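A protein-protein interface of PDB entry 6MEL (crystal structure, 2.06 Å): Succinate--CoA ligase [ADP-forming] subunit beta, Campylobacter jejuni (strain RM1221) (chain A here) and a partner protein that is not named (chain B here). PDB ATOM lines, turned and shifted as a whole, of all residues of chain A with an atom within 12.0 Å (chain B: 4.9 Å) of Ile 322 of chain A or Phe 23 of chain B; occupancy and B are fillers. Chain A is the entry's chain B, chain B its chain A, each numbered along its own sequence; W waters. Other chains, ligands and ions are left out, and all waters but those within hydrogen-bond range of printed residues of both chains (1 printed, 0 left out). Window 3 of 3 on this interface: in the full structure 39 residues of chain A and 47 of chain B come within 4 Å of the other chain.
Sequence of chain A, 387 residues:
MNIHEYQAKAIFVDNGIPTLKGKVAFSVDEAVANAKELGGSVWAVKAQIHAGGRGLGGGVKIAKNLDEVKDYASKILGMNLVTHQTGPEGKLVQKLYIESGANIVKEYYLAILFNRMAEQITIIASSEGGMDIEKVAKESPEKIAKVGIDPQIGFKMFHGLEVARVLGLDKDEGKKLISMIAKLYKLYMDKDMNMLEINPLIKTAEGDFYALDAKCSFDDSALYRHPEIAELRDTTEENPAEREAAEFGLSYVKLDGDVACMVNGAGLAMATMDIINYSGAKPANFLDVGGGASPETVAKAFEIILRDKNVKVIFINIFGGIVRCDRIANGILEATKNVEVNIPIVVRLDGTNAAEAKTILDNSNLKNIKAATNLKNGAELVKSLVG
Among the printed residues, pairs that only touch across the chains: Gly 321 of chain A with Pro 139 of chain B, Ile 322 of chain A with Phe 23 of chain B, Ile 322 of chain A with Gln 27 of chain B, Ile 322 of chain A with Ile 137 of chain B, Ile 322 of chain A with Met 138 of chain B and Ile 322 of chain A with Pro 139 of chain B.
Of the 26 printed residues of chain A, 2 touch a printed residue of chain B. Printed residues of chain A that touch a printed residue of chain B: Gly 321 and Ile 322. Hydrophobic or aromatic side chains of chain A within 4 Å of the printed part of chain B: Ile 322. Of the 13 printed residues of chain B, 5 touch a printed residue of chain A. Printed residues of chain B that touch a printed residue of chain A: Phe 23, Gln 27, Ile 137, Met 138 and Pro 139.
The backbone carbonyl oxygen (O) of Met 138 of chain B sits at hydrogen-bond distance from the side-chain amino group (NZ) of Lys 134 of chain B (2.8 Å). O of Gly 321 of chain A lies within hydrogen-bond range of OG1 of Thr 352 of chain A (2.6 Å).
Water W1 lies within hydrogen-bond range of the backbone carbonyl oxygen of Ile 322 of chain A and the side-chain amide nitrogen of Gln 27 of chain B.
Gly 265 of chain A touches none of the printed residues of chain B. Printed residues of chain B within 4 Å of Gly 321 of chain A: Pro 139 (3.6 Å). Of the printed residues of chain B, Ile 322 of chain A touches Phe 23 (3.5 Å), Gln 27 (3.4 Å), Ile 137 (3.3 Å), Met 138 (3.98 Å) and Pro 139 (3.98 Å). No residue of chain A comes within 4 Å of Ala 21 of chain B. No residue of chain A comes within 4 Å of Thr 22 of chain B. Phe 23 of chain B touches just one residue of chain A: Ile 322 (3.5 Å). No residue of chain A comes within 4 Å of His 24 of chain B. No residue of chain A comes within 4 Å of Ala 25 of chain B. Of chain A, only Ile 322 comes within 4 Å of Gln 27 of chain B. Of chain A, only Ile 322 comes within 4 Å of Ile 137 of chain B. Of the printed residues of chain A, Met 138 of chain B touches Ile 322. Of chain A, only Gly 321 and Ile 322 come within 4 Å of Pro 139 of chain B. The nearest residue of chain A that does not touch Phe 23 of chain B is Val 323 of chain A (7.0 Å). The nearest printed residue of chain B that does not touch Gly 321 of chain A is Met 138 of chain B (6.2 Å).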
ATOM      1  N   ASN A 264      10.976  -7.142   6.996  1.00  0.00           N
ATOM      2  CA  ASN A 264      11.167  -6.638   5.657  1.00  0.00           C
ATOM      3  C   ASN A 264      10.591  -7.636   4.624  1.00  0.00           C
ATOM      4  O   ASN A 264      11.014  -8.806   4.550  1.00  0.00           O
ATOM      5  CB  ASN A 264      12.626  -6.263   5.384  1.00  0.00           C
ATOM      6  CG  ASN A 264      13.635  -7.397   5.396  1.00  0.00           C
ATOM      7  OD1 ASN A 264      13.493  -8.359   6.173  1.00  0.00           O
ATOM      8  ND2 ASN A 264      14.696  -7.229   4.594  1.00  0.00           N
ATOM      9  N   GLY A 265       9.650  -7.138   3.807  1.00  0.00           N
ATOM     10  CA  GLY A 265       9.022  -7.888   2.718  1.00  0.00           C
ATOM     11  C   GLY A 265       7.671  -8.458   3.175  1.00  0.00           C
ATOM     12  O   GLY A 265       7.545  -9.017   4.272  1.00  0.00           O
ATOM     13  N   LEU A 268       7.465 -12.292   3.989  1.00  0.00           N
ATOM     14  CA  LEU A 268       8.103 -12.645   5.259  1.00  0.00           C
ATOM     15  C   LEU A 268       7.330 -12.022   6.421  1.00  0.00           C
ATOM     16  O   LEU A 268       7.258 -12.600   7.516  1.00  0.00           O
ATOM     17  CB  LEU A 268       9.556 -12.189   5.250  1.00  0.00           C
ATOM     18  CG  LEU A 268      10.380 -12.538   6.486  1.00  0.00           C
ATOM     19  CD1 LEU A 268      10.589 -14.049   6.580  1.00  0.00           C
ATOM     20  CD2 LEU A 268      11.757 -11.872   6.408  1.00  0.00           C
ATOM     21  N   VAL A 289       8.751  -3.053   6.498  1.00  0.00           N
ATOM     22  CA  VAL A 289       9.688  -1.939   6.452  1.00  0.00           C
ATOM     23  C   VAL A 289      10.904  -2.447   5.677  1.00  0.00           C
ATOM     24  O   VAL A 289      11.372  -3.549   5.934  1.00  0.00           O
ATOM     25  CB  VAL A 289      10.099  -1.460   7.856  1.00  0.00           C
ATOM     26  CG1 VAL A 289      10.606  -2.593   8.736  1.00  0.00           C
ATOM     27  CG2 VAL A 289      11.179  -0.388   7.785  1.00  0.00           C
ATOM     28  N   GLY A 290      11.457  -1.620   4.802  1.00  0.00           N
ATOM     29  CA  GLY A 290      12.648  -2.043   4.055  1.00  0.00           C
ATOM     30  C   GLY A 290      13.832  -2.282   4.989  1.00  0.00           C
ATOM     31  O   GLY A 290      14.062  -1.536   5.953  1.00  0.00           O
ATOM     32  N   GLY A 291      14.630  -3.300   4.687  1.00  0.00           N
ATOM     33  CA  GLY A 291      15.811  -3.552   5.479  1.00  0.00           C
ATOM     34  C   GLY A 291      16.786  -2.395   5.384  1.00  0.00           C
ATOM     35  O   GLY A 291      17.559  -2.198   6.253  1.00  0.00           O
ATOM     36  N   GLY A 292      16.763  -1.701   4.250  1.00  0.00           N
ATOM     37  CA  GLY A 292      17.560  -0.517   3.986  1.00  0.00           C
ATOM     38  C   GLY A 292      16.945   0.763   4.524  1.00  0.00           C
ATOM     39  O   GLY A 292      17.479   1.808   4.270  1.00  0.00           O
ATOM     40  N   ALA A 293      15.808   0.701   5.225  1.00  0.00           N
ATOM     41  CA  ALA A 293      15.176   1.932   5.727  1.00  0.00           C
ATOM     42  C   ALA A 293      16.177   2.696   6.615  1.00  0.00           C
ATOM     43  O   ALA A 293      17.015   2.076   7.337  1.00  0.00           O
ATOM     44  CB  ALA A 293      13.930   1.613   6.520  1.00  0.00           C
ATOM     45  N   ILE A 318      14.185  -9.662  10.274  1.00  0.00           N
ATOM     46  CA  ILE A 318      14.655  -8.993   9.082  1.00  0.00           C
ATOM     47  C   ILE A 318      15.737  -9.857   8.446  1.00  0.00           C
ATOM     48  O   ILE A 318      16.716 -10.272   9.114  1.00  0.00           O
ATOM     49  CB  ILE A 318      15.152  -7.570   9.417  1.00  0.00           C
ATOM     50  CG1 ILE A 318      13.958  -6.652   9.735  1.00  0.00           C
ATOM     51  CG2 ILE A 318      16.028  -7.027   8.283  1.00  0.00           C
ATOM     52  CD1 ILE A 318      14.330  -5.248  10.149  1.00  0.00           C
ATOM     53  N   PHE A 319      15.594 -10.066   7.141  1.00  0.00           N
ATOM     54  CA  PHE A 319      16.588 -10.778   6.355  1.00  0.00           C
ATOM     55  C   PHE A 319      17.389  -9.742   5.561  1.00  0.00           C
ATOM     56  O   PHE A 319      16.890  -9.139   4.596  1.00  0.00           O
ATOM     57  CB  PHE A 319      15.945 -11.822   5.451  1.00  0.00           C
ATOM     58  CG  PHE A 319      16.925 -12.837   4.917  1.00  0.00           C
ATOM     59  CD1 PHE A 319      17.829 -12.491   3.932  1.00  0.00           C
ATOM     60  CD2 PHE A 319      17.010 -14.107   5.486  1.00  0.00           C
ATOM     61  CE1 PHE A 319      18.786 -13.409   3.512  1.00  0.00           C
ATOM     62  CE2 PHE A 319      17.944 -15.033   5.034  1.00  0.00           C
ATOM     63  CZ  PHE A 319      18.830 -14.676   4.061  1.00  0.00           C
ATOM     64  N   GLY A 320      18.623  -9.503   6.008  1.00  0.00           N
ATOM     65  CA  GLY A 320      19.549  -8.633   5.274  1.00  0.00           C
ATOM     66  C   GLY A 320      20.224  -9.400   4.142  1.00  0.00           C
ATOM     67  O   GLY A 320      21.117 -10.179   4.373  1.00  0.00           O
ATOM     68  N   GLY A 321      19.781  -9.178   2.910  1.00  0.00           N
ATOM     69  CA  GLY A 321      20.347  -9.846   1.769  1.00  0.00           C
ATOM     70  C   GLY A 321      21.375  -8.941   1.103  1.00  0.00           C
ATOM     71  O   GLY A 321      22.566  -9.037   1.379  1.00  0.00           O
ATOM     72  N   ILE A 322      20.880  -8.021   0.271  1.00  0.00           N
ATOM     73  CA  ILE A 322      21.663  -6.926  -0.285  1.00  0.00           C
ATOM     74  C   ILE A 322      22.078  -5.971   0.842  1.00  0.00           C
ATOM     75  O   ILE A 322      23.146  -5.391   0.759  1.00  0.00           O
ATOM     76  CB  ILE A 322      20.867  -6.164  -1.363  1.00  0.00           C
ATOM     77  CG1 ILE A 322      20.411  -7.082  -2.496  1.00  0.00           C
ATOM     78  CG2 ILE A 322      21.658  -4.968  -1.890  1.00  0.00           C
ATOM     79  CD1 ILE A 322      21.505  -7.896  -3.138  1.00  0.00           C
ATOM     80  N   VAL A 323      21.209  -5.749   1.843  1.00  0.00           N
ATOM     81  CA  VAL A 323      21.540  -4.864   2.961  1.00  0.00           C
ATOM     82  C   VAL A 323      22.205  -5.699   4.055  1.00  0.00           C
ATOM     83  O   VAL A 323      21.732  -6.747   4.390  1.00  0.00           O
ATOM     84  CB  VAL A 323      20.300  -4.130   3.502  1.00  0.00           C
ATOM     85  CG1 VAL A 323      20.658  -3.222   4.672  1.00  0.00           C
ATOM     86  CG2 VAL A 323      19.639  -3.311   2.399  1.00  0.00           C
ATOM     87  N   ARG A 324      23.316  -5.214   4.585  1.00  0.00           N
ATOM     88  CA  ARG A 324      24.111  -5.923   5.606  1.00  0.00           C
ATOM     89  C   ARG A 324      23.415  -5.840   6.965  1.00  0.00           C
ATOM     90  O   ARG A 324      22.964  -4.764   7.370  1.00  0.00           O
ATOM     91  CB  ARG A 324      25.505  -5.315   5.739  1.00  0.00           C
ATOM     92  CG  ARG A 324      26.329  -5.300   4.460  1.00  0.00           C
ATOM     93  CD  ARG A 324      27.473  -4.289   4.499  1.00  0.00           C
ATOM     94  NE  ARG A 324      28.258  -4.510   5.706  1.00  0.00           N
ATOM     95  CZ  ARG A 324      29.286  -3.769   6.108  1.00  0.00           C
ATOM     96  NH1 ARG A 324      29.634  -2.673   5.450  1.00  0.00           N
ATOM     97  NH2 ARG A 324      29.959  -4.133   7.181  1.00  0.00           N
ATOM     98  N   CYS A 325      23.317  -6.988   7.638  1.00  0.00           N
ATOM     99  CA  CYS A 325      22.601  -7.096   8.888  1.00  0.00           C
ATOM    100  C   CYS A 325      23.248  -6.209   9.955  1.00  0.00           C
ATOM    101  O   CYS A 325      22.575  -5.775  10.845  1.00  0.00           O
ATOM    102  CB  CYS A 325      22.574  -8.533   9.396  1.00  0.00           C
ATOM    103  SG  CYS A 325      21.417  -9.630   8.526  1.00  0.00           S
ATOM    104  N   ASP A 326      24.568  -5.977   9.867  1.00  0.00           N
ATOM    105  CA  ASP A 326      25.280  -5.174  10.897  1.00  0.00           C
ATOM    106  C   ASP A 326      24.839  -3.727  10.778  1.00  0.00           C
ATOM    107  O   ASP A 326      24.659  -3.044  11.789  1.00  0.00           O
ATOM    108  CB  ASP A 326      26.807  -5.323  10.870  1.00  0.00           C
ATOM    109  CG  ASP A 326      27.467  -5.119   9.523  1.00  0.00           C
ATOM    110  OD1 ASP A 326      26.841  -5.366   8.482  1.00  0.00           O
ATOM    111  OD2 ASP A 326      28.601  -4.718   9.527  1.00  0.00           O
ATOM    112  N   ARG A 327      24.589  -3.272   9.555  1.00  0.00           N
ATOM    113  CA  ARG A 327      24.085  -1.925   9.413  1.00  0.00           C
ATOM    114  C   ARG A 327      22.622  -1.869   9.886  1.00  0.00           C
ATOM    115  O   ARG A 327      22.216  -0.882  10.486  1.00  0.00           O
ATOM    116  CB  ARG A 327      24.322  -1.442   7.987  1.00  0.00           C
ATOM    117  CG  ARG A 327      25.799  -1.340   7.630  1.00  0.00           C
ATOM    118  CD  ARG A 327      25.894  -0.907   6.186  1.00  0.00           C
ATOM    119  NE  ARG A 327      27.254  -0.629   5.786  1.00  0.00           N
ATOM    120  CZ  ARG A 327      27.573  -0.216   4.576  1.00  0.00           C
ATOM    121  NH1 ARG A 327      26.621  -0.043   3.679  1.00  0.00           N
ATOM    122  NH2 ARG A 327      28.832   0.020   4.265  1.00  0.00           N
ATOM    123  N   ILE A 328      21.856  -2.945   9.694  1.00  0.00           N
ATOM    124  CA  ILE A 328      20.460  -2.949  10.201  1.00  0.00           C
ATOM    125  C   ILE A 328      20.474  -2.863  11.738  1.00  0.00           C
ATOM    126  O   ILE A 328      19.675  -2.113  12.364  1.00  0.00           O
ATOM    127  CB  ILE A 328      19.681  -4.158   9.648  1.00  0.00           C
ATOM    128  CG1 ILE A 328      19.494  -3.990   8.138  1.00  0.00           C
ATOM    129  CG2 ILE A 328      18.352  -4.315  10.356  1.00  0.00           C
ATOM    130  CD1 ILE A 328      19.212  -5.296   7.410  1.00  0.00           C
ATOM    131  N   ALA A 329      21.398  -3.606  12.355  1.00  0.00           N
ATOM    132  CA  ALA A 329      21.515  -3.656  13.819  1.00  0.00           C
ATOM    133  C   ALA A 329      21.833  -2.267  14.389  1.00  0.00           C
ATOM    134  O   ALA A 329      21.181  -1.820  15.366  1.00  0.00           O
ATOM    135  CB  ALA A 329      22.564  -4.664  14.228  1.00  0.00           C
ATOM    136  N   LEU A 349      17.948 -11.230  13.038  1.00  0.00           N
ATOM    137  CA  LEU A 349      18.548 -10.763  11.839  1.00  0.00           C
ATOM    138  C   LEU A 349      19.275 -11.942  11.221  1.00  0.00           C
ATOM    139  O   LEU A 349      20.084 -12.598  11.909  1.00  0.00           O
ATOM    140  CB  LEU A 349      19.549  -9.644  12.125  1.00  0.00           C
ATOM    141  CG  LEU A 349      18.967  -8.381  12.750  1.00  0.00           C
ATOM    142  CD1 LEU A 349      20.048  -7.368  13.059  1.00  0.00           C
ATOM    143  CD2 LEU A 349      17.937  -7.772  11.832  1.00  0.00           C
ATOM    144  N   ASP A 350      19.038 -12.177   9.931  1.00  0.00           N
ATOM    145  CA  ASP A 350      19.766 -13.251   9.255  1.00  0.00           C
ATOM    146  C   ASP A 350      20.132 -12.815   7.841  1.00  0.00           C
ATOM    147  O   ASP A 350      19.596 -11.855   7.322  1.00  0.00           O
ATOM    148  CB  ASP A 350      18.979 -14.557   9.280  1.00  0.00           C
ATOM    149  CG  ASP A 350      19.873 -15.793   9.245  1.00  0.00           C
ATOM    150  OD1 ASP A 350      21.117 -15.626   9.124  1.00  0.00           O
ATOM    151  OD2 ASP A 350      19.317 -16.898   9.311  1.00  0.00           O
ATOM    152  N   GLY A 351      21.095 -13.519   7.237  1.00  0.00           N
ATOM    153  CA  GLY A 351      21.661 -13.125   5.946  1.00  0.00           C
ATOM    154  C   GLY A 351      23.067 -12.580   6.079  1.00  0.00           C
ATOM    155  O   GLY A 351      23.861 -13.075   6.885  1.00  0.00           O
ATOM    156  N   THR A 352      23.347 -11.531   5.303  1.00  0.00           N
ATOM    157  CA  THR A 352      24.659 -10.926   5.190  1.00  0.00           C
ATOM    158  C   THR A 352      25.105 -10.382   6.555  1.00  0.00           C
ATOM    159  O   THR A 352      24.417  -9.570   7.142  1.00  0.00           O
ATOM    160  CB  THR A 352      24.620  -9.824   4.124  1.00  0.00           C
ATOM    161  OG1 THR A 352      24.069 -10.403   2.943  1.00  0.00           O
ATOM    162  CG2 THR A 352      25.971  -9.204   3.827  1.00  0.00           C
ATOM    163  N   ASN A 353      26.259 -10.858   7.043  1.00  0.00           N
ATOM    164  CA  ASN A 353      26.908 -10.379   8.271  1.00  0.00           C
ATOM    165  C   ASN A 353      25.997 -10.560   9.483  1.00  0.00           C
ATOM    166  O   ASN A 353      26.018  -9.733  10.400  1.00  0.00           O
ATOM    167  CB  ASN A 353      27.312  -8.901   8.188  1.00  0.00           C
ATOM    168  CG  ASN A 353      28.449  -8.636   7.216  1.00  0.00           C
ATOM    169  OD1 ASN A 353      29.068  -9.565   6.718  1.00  0.00           O
ATOM    170  ND2 ASN A 353      28.747  -7.377   6.954  1.00  0.00           N
ATOM    171  N   ALA A 354      25.207 -11.633   9.472  1.00  0.00           N
ATOM    172  CA  ALA A 354      24.290 -11.927  10.541  1.00  0.00           C
ATOM    173  C   ALA A 354      25.057 -12.050  11.863  1.00  0.00           C
ATOM    174  O   ALA A 354      24.577 -11.560  12.908  1.00  0.00           O
ATOM    175  CB  ALA A 354      23.534 -13.203  10.251  1.00  0.00           C
ATOM    176  N   LYS B  19      19.893   4.411 -11.206  1.00  0.00           N
ATOM    177  CA  LYS B  19      20.793   4.210 -10.080  1.00  0.00           C
ATOM    178  C   LYS B  19      20.699   2.773  -9.544  1.00  0.00           C
ATOM    179  O   LYS B  19      21.694   2.063  -9.399  1.00  0.00           O
ATOM    180  CB  LYS B  19      20.442   5.214  -8.982  1.00  0.00           C
ATOM    181  CG  LYS B  19      21.628   5.925  -8.367  1.00  0.00           C
ATOM    182  CD  LYS B  19      21.316   6.534  -7.013  1.00  0.00           C
ATOM    183  CE  LYS B  19      22.505   6.510  -6.073  1.00  0.00           C
ATOM    184  NZ  LYS B  19      22.093   6.849  -4.691  1.00  0.00           N
ATOM    185  N   GLU B  20      19.485   2.365  -9.219  1.00  0.00           N
ATOM    186  CA  GLU B  20      19.202   1.038  -8.648  1.00  0.00           C
ATOM    187  C   GLU B  20      19.598  -0.056  -9.636  1.00  0.00           C
ATOM    188  O   GLU B  20      20.216  -1.018  -9.285  1.00  0.00           O
ATOM    189  CB  GLU B  20      17.705   0.871  -8.384  1.00  0.00           C
ATOM    190  CG  GLU B  20      17.257   1.077  -6.959  1.00  0.00           C
ATOM    191  CD  GLU B  20      15.985   0.278  -6.673  1.00  0.00           C
ATOM    192  OE1 GLU B  20      15.952  -0.445  -5.662  1.00  0.00           O
ATOM    193  OE2 GLU B  20      15.051   0.322  -7.498  1.00  0.00           O
ATOM    194  N   ALA B  21      19.155   0.100 -10.878  1.00  0.00           N
ATOM    195  CA  ALA B  21      19.452  -0.818 -11.950  1.00  0.00           C
ATOM    196  C   ALA B  21      20.967  -0.988 -12.098  1.00  0.00           C
ATOM    197  O   ALA B  21      21.445  -2.112 -12.310  1.00  0.00           O
ATOM    198  CB  ALA B  21      18.872  -0.318 -13.245  1.00  0.00           C
ATOM    199  N   THR B  22      21.700   0.130 -11.991  1.00  0.00           N
ATOM    200  CA  THR B  22      23.175   0.114 -12.142  1.00  0.00           C
ATOM    201  C   THR B  22      23.797  -0.742 -11.013  1.00  0.00           C
ATOM    202  O   THR B  22      24.601  -1.615 -11.260  1.00  0.00           O
ATOM    203  CB  THR B  22      23.755   1.542 -12.169  1.00  0.00           C
ATOM    204  OG1 THR B  22      23.237   2.220 -13.319  1.00  0.00           O
ATOM    205  CG2 THR B  22      25.280   1.550 -12.188  1.00  0.00           C
ATOM    206  N   PHE B  23      23.389  -0.465  -9.775  1.00  0.00           N
ATOM    207  CA  PHE B  23      23.829  -1.194  -8.616  1.00  0.00           C
ATOM    208  C   PHE B  23      23.595  -2.702  -8.828  1.00  0.00           C
ATOM    209  O   PHE B  23      24.525  -3.489  -8.690  1.00  0.00           O
ATOM    210  CB  PHE B  23      23.088  -0.693  -7.371  1.00  0.00           C
ATOM    211  CG  PHE B  23      23.448  -1.452  -6.125  1.00  0.00           C
ATOM    212  CD1 PHE B  23      24.515  -1.042  -5.323  1.00  0.00           C
ATOM    213  CD2 PHE B  23      22.765  -2.612  -5.788  1.00  0.00           C
ATOM    214  CE1 PHE B  23      24.866  -1.773  -4.187  1.00  0.00           C
ATOM    215  CE2 PHE B  23      23.125  -3.358  -4.670  1.00  0.00           C
ATOM    216  CZ  PHE B  23      24.163  -2.921  -3.854  1.00  0.00           C
ATOM    217  N   HIS B  24      22.357  -3.106  -9.191  1.00  0.00           N
ATOM    218  CA  HIS B  24      22.042  -4.504  -9.291  1.00  0.00           C
ATOM    219  C   HIS B  24      22.722  -5.132 -10.511  1.00  0.00           C
ATOM    220  O   HIS B  24      23.206  -6.250 -10.408  1.00  0.00           O
ATOM    221  CB  HIS B  24      20.530  -4.746  -9.257  1.00  0.00           C
ATOM    222  CG  HIS B  24      19.964  -4.444  -7.913  1.00  0.00           C
ATOM    223  ND1 HIS B  24      20.220  -5.243  -6.818  1.00  0.00           N
ATOM    224  CD2 HIS B  24      19.209  -3.412  -7.475  1.00  0.00           C
ATOM    225  CE1 HIS B  24      19.588  -4.738  -5.771  1.00  0.00           C
ATOM    226  NE2 HIS B  24      18.989  -3.595  -6.140  1.00  0.00           N
ATOM    227  N   ALA B  25      22.710  -4.448 -11.654  1.00  0.00           N
ATOM    228  CA  ALA B  25      23.364  -4.957 -12.904  1.00  0.00           C
ATOM    229  C   ALA B  25      24.834  -5.311 -12.633  1.00  0.00           C
ATOM    230  O   ALA B  25      25.323  -6.366 -13.088  1.00  0.00           O
ATOM    231  CB  ALA B  25      23.271  -3.970 -14.048  1.00  0.00           C
ATOM    232  N   GLU B  26      25.509  -4.486 -11.836  1.00  0.00           N
ATOM    233  CA  GLU B  26      26.927  -4.692 -11.495  1.00  0.00           C
ATOM    234  C   GLU B  26      27.054  -5.972 -10.660  1.00  0.00           C
ATOM    235  O   GLU B  26      27.880  -6.832 -10.939  1.00  0.00           O
ATOM    236  CB  GLU B  26      27.443  -3.440 -10.774  1.00  0.00           C
ATOM    237  CG  GLU B  26      28.948  -3.398 -10.553  1.00  0.00           C
ATOM    238  CD  GLU B  26      29.423  -2.056 -10.011  1.00  0.00           C
ATOM    239  OE1 GLU B  26      28.937  -1.640  -8.939  1.00  0.00           O
ATOM    240  OE2 GLU B  26      30.247  -1.409 -10.682  1.00  0.00           O
ATOM    241  N   GLN B  27      26.218  -6.081  -9.609  1.00  0.00           N
ATOM    242  CA  GLN B  27      26.214  -7.312  -8.791  1.00  0.00           C
ATOM    243  C   GLN B  27      25.867  -8.540  -9.653  1.00  0.00           C
ATOM    244  O   GLN B  27      26.486  -9.573  -9.492  1.00  0.00           O
ATOM    245  CB  GLN B  27      25.277  -7.194  -7.601  1.00  0.00           C
ATOM    246  CG  GLN B  27      25.724  -6.129  -6.610  1.00  0.00           C
ATOM    247  CD  GLN B  27      25.175  -6.410  -5.236  1.00  0.00           C
ATOM    248  OE1 GLN B  27      24.212  -7.160  -5.055  1.00  0.00           O
ATOM    249  NE2 GLN B  27      25.852  -5.866  -4.248  1.00  0.00           N
ATOM    250  N   LYS B 134      22.460 -14.510 -12.040  1.00  0.00           N
ATOM    251  CA  LYS B 134      21.303 -13.962 -11.362  1.00  0.00           C
ATOM    252  C   LYS B 134      20.778 -12.755 -12.147  1.00  0.00           C
ATOM    253  O   LYS B 134      21.550 -11.951 -12.686  1.00  0.00           O
ATOM    254  CB  LYS B 134      21.654 -13.678  -9.899  1.00  0.00           C
ATOM    255  CG  LYS B 134      22.158 -12.285  -9.578  1.00  0.00           C
ATOM    256  CD  LYS B 134      22.459 -12.114  -8.124  1.00  0.00           C
ATOM    257  CE  LYS B 134      22.889 -10.716  -7.709  1.00  0.00           C
ATOM    258  NZ  LYS B 134      21.708  -9.834  -7.530  1.00  0.00           N
ATOM    259  N   ILE B 137      17.500  -8.879  -7.977  1.00  0.00           N
ATOM    260  CA  ILE B 137      17.932  -8.150  -6.798  1.00  0.00           C
ATOM    261  C   ILE B 137      18.213  -9.122  -5.643  1.00  0.00           C
ATOM    262  O   ILE B 137      18.385  -8.705  -4.487  1.00  0.00           O
ATOM    263  CB  ILE B 137      16.881  -7.106  -6.380  1.00  0.00           C
ATOM    264  CG1 ILE B 137      15.575  -7.773  -5.939  1.00  0.00           C
ATOM    265  CG2 ILE B 137      16.666  -6.055  -7.472  1.00  0.00           C
ATOM    266  CD1 ILE B 137      14.557  -6.797  -5.314  1.00  0.00           C
ATOM    267  N   MET B 138      18.252 -10.431  -5.923  1.00  0.00           N
ATOM    268  CA  MET B 138      18.474 -11.375  -4.823  1.00  0.00           C
ATOM    269  C   MET B 138      19.952 -11.393  -4.410  1.00  0.00           C
ATOM    270  O   MET B 138      20.837 -11.211  -5.246  1.00  0.00           O
ATOM    271  CB  MET B 138      18.007 -12.784  -5.191  1.00  0.00           C
ATOM    272  CG  MET B 138      18.789 -13.420  -6.314  1.00  0.00           C
ATOM    273  SD  MET B 138      18.463 -12.665  -7.946  1.00  0.00           S
ATOM    274  CE  MET B 138      16.784 -13.265  -8.163  1.00  0.00           C
ATOM    275  N   PRO B 139      20.242 -11.669  -3.109  1.00  0.00           N
ATOM    276  CA  PRO B 139      21.610 -11.841  -2.606  1.00  0.00           C
ATOM    277  C   PRO B 139      22.223 -13.163  -3.093  1.00  0.00           C
ATOM    278  O   PRO B 139      21.834 -14.263  -2.651  1.00  0.00           O
ATOM    279  CB  PRO B 139      21.449 -11.831  -1.088  1.00  0.00           C
ATOM    280  CG  PRO B 139      20.025 -12.384  -0.862  1.00  0.00           C
ATOM    281  CD  PRO B 139      19.232 -11.835  -2.040  1.00  0.00           C
HETATM  282  O   HOH W   1      24.992  -5.857  -1.375  1.00  0.00           O
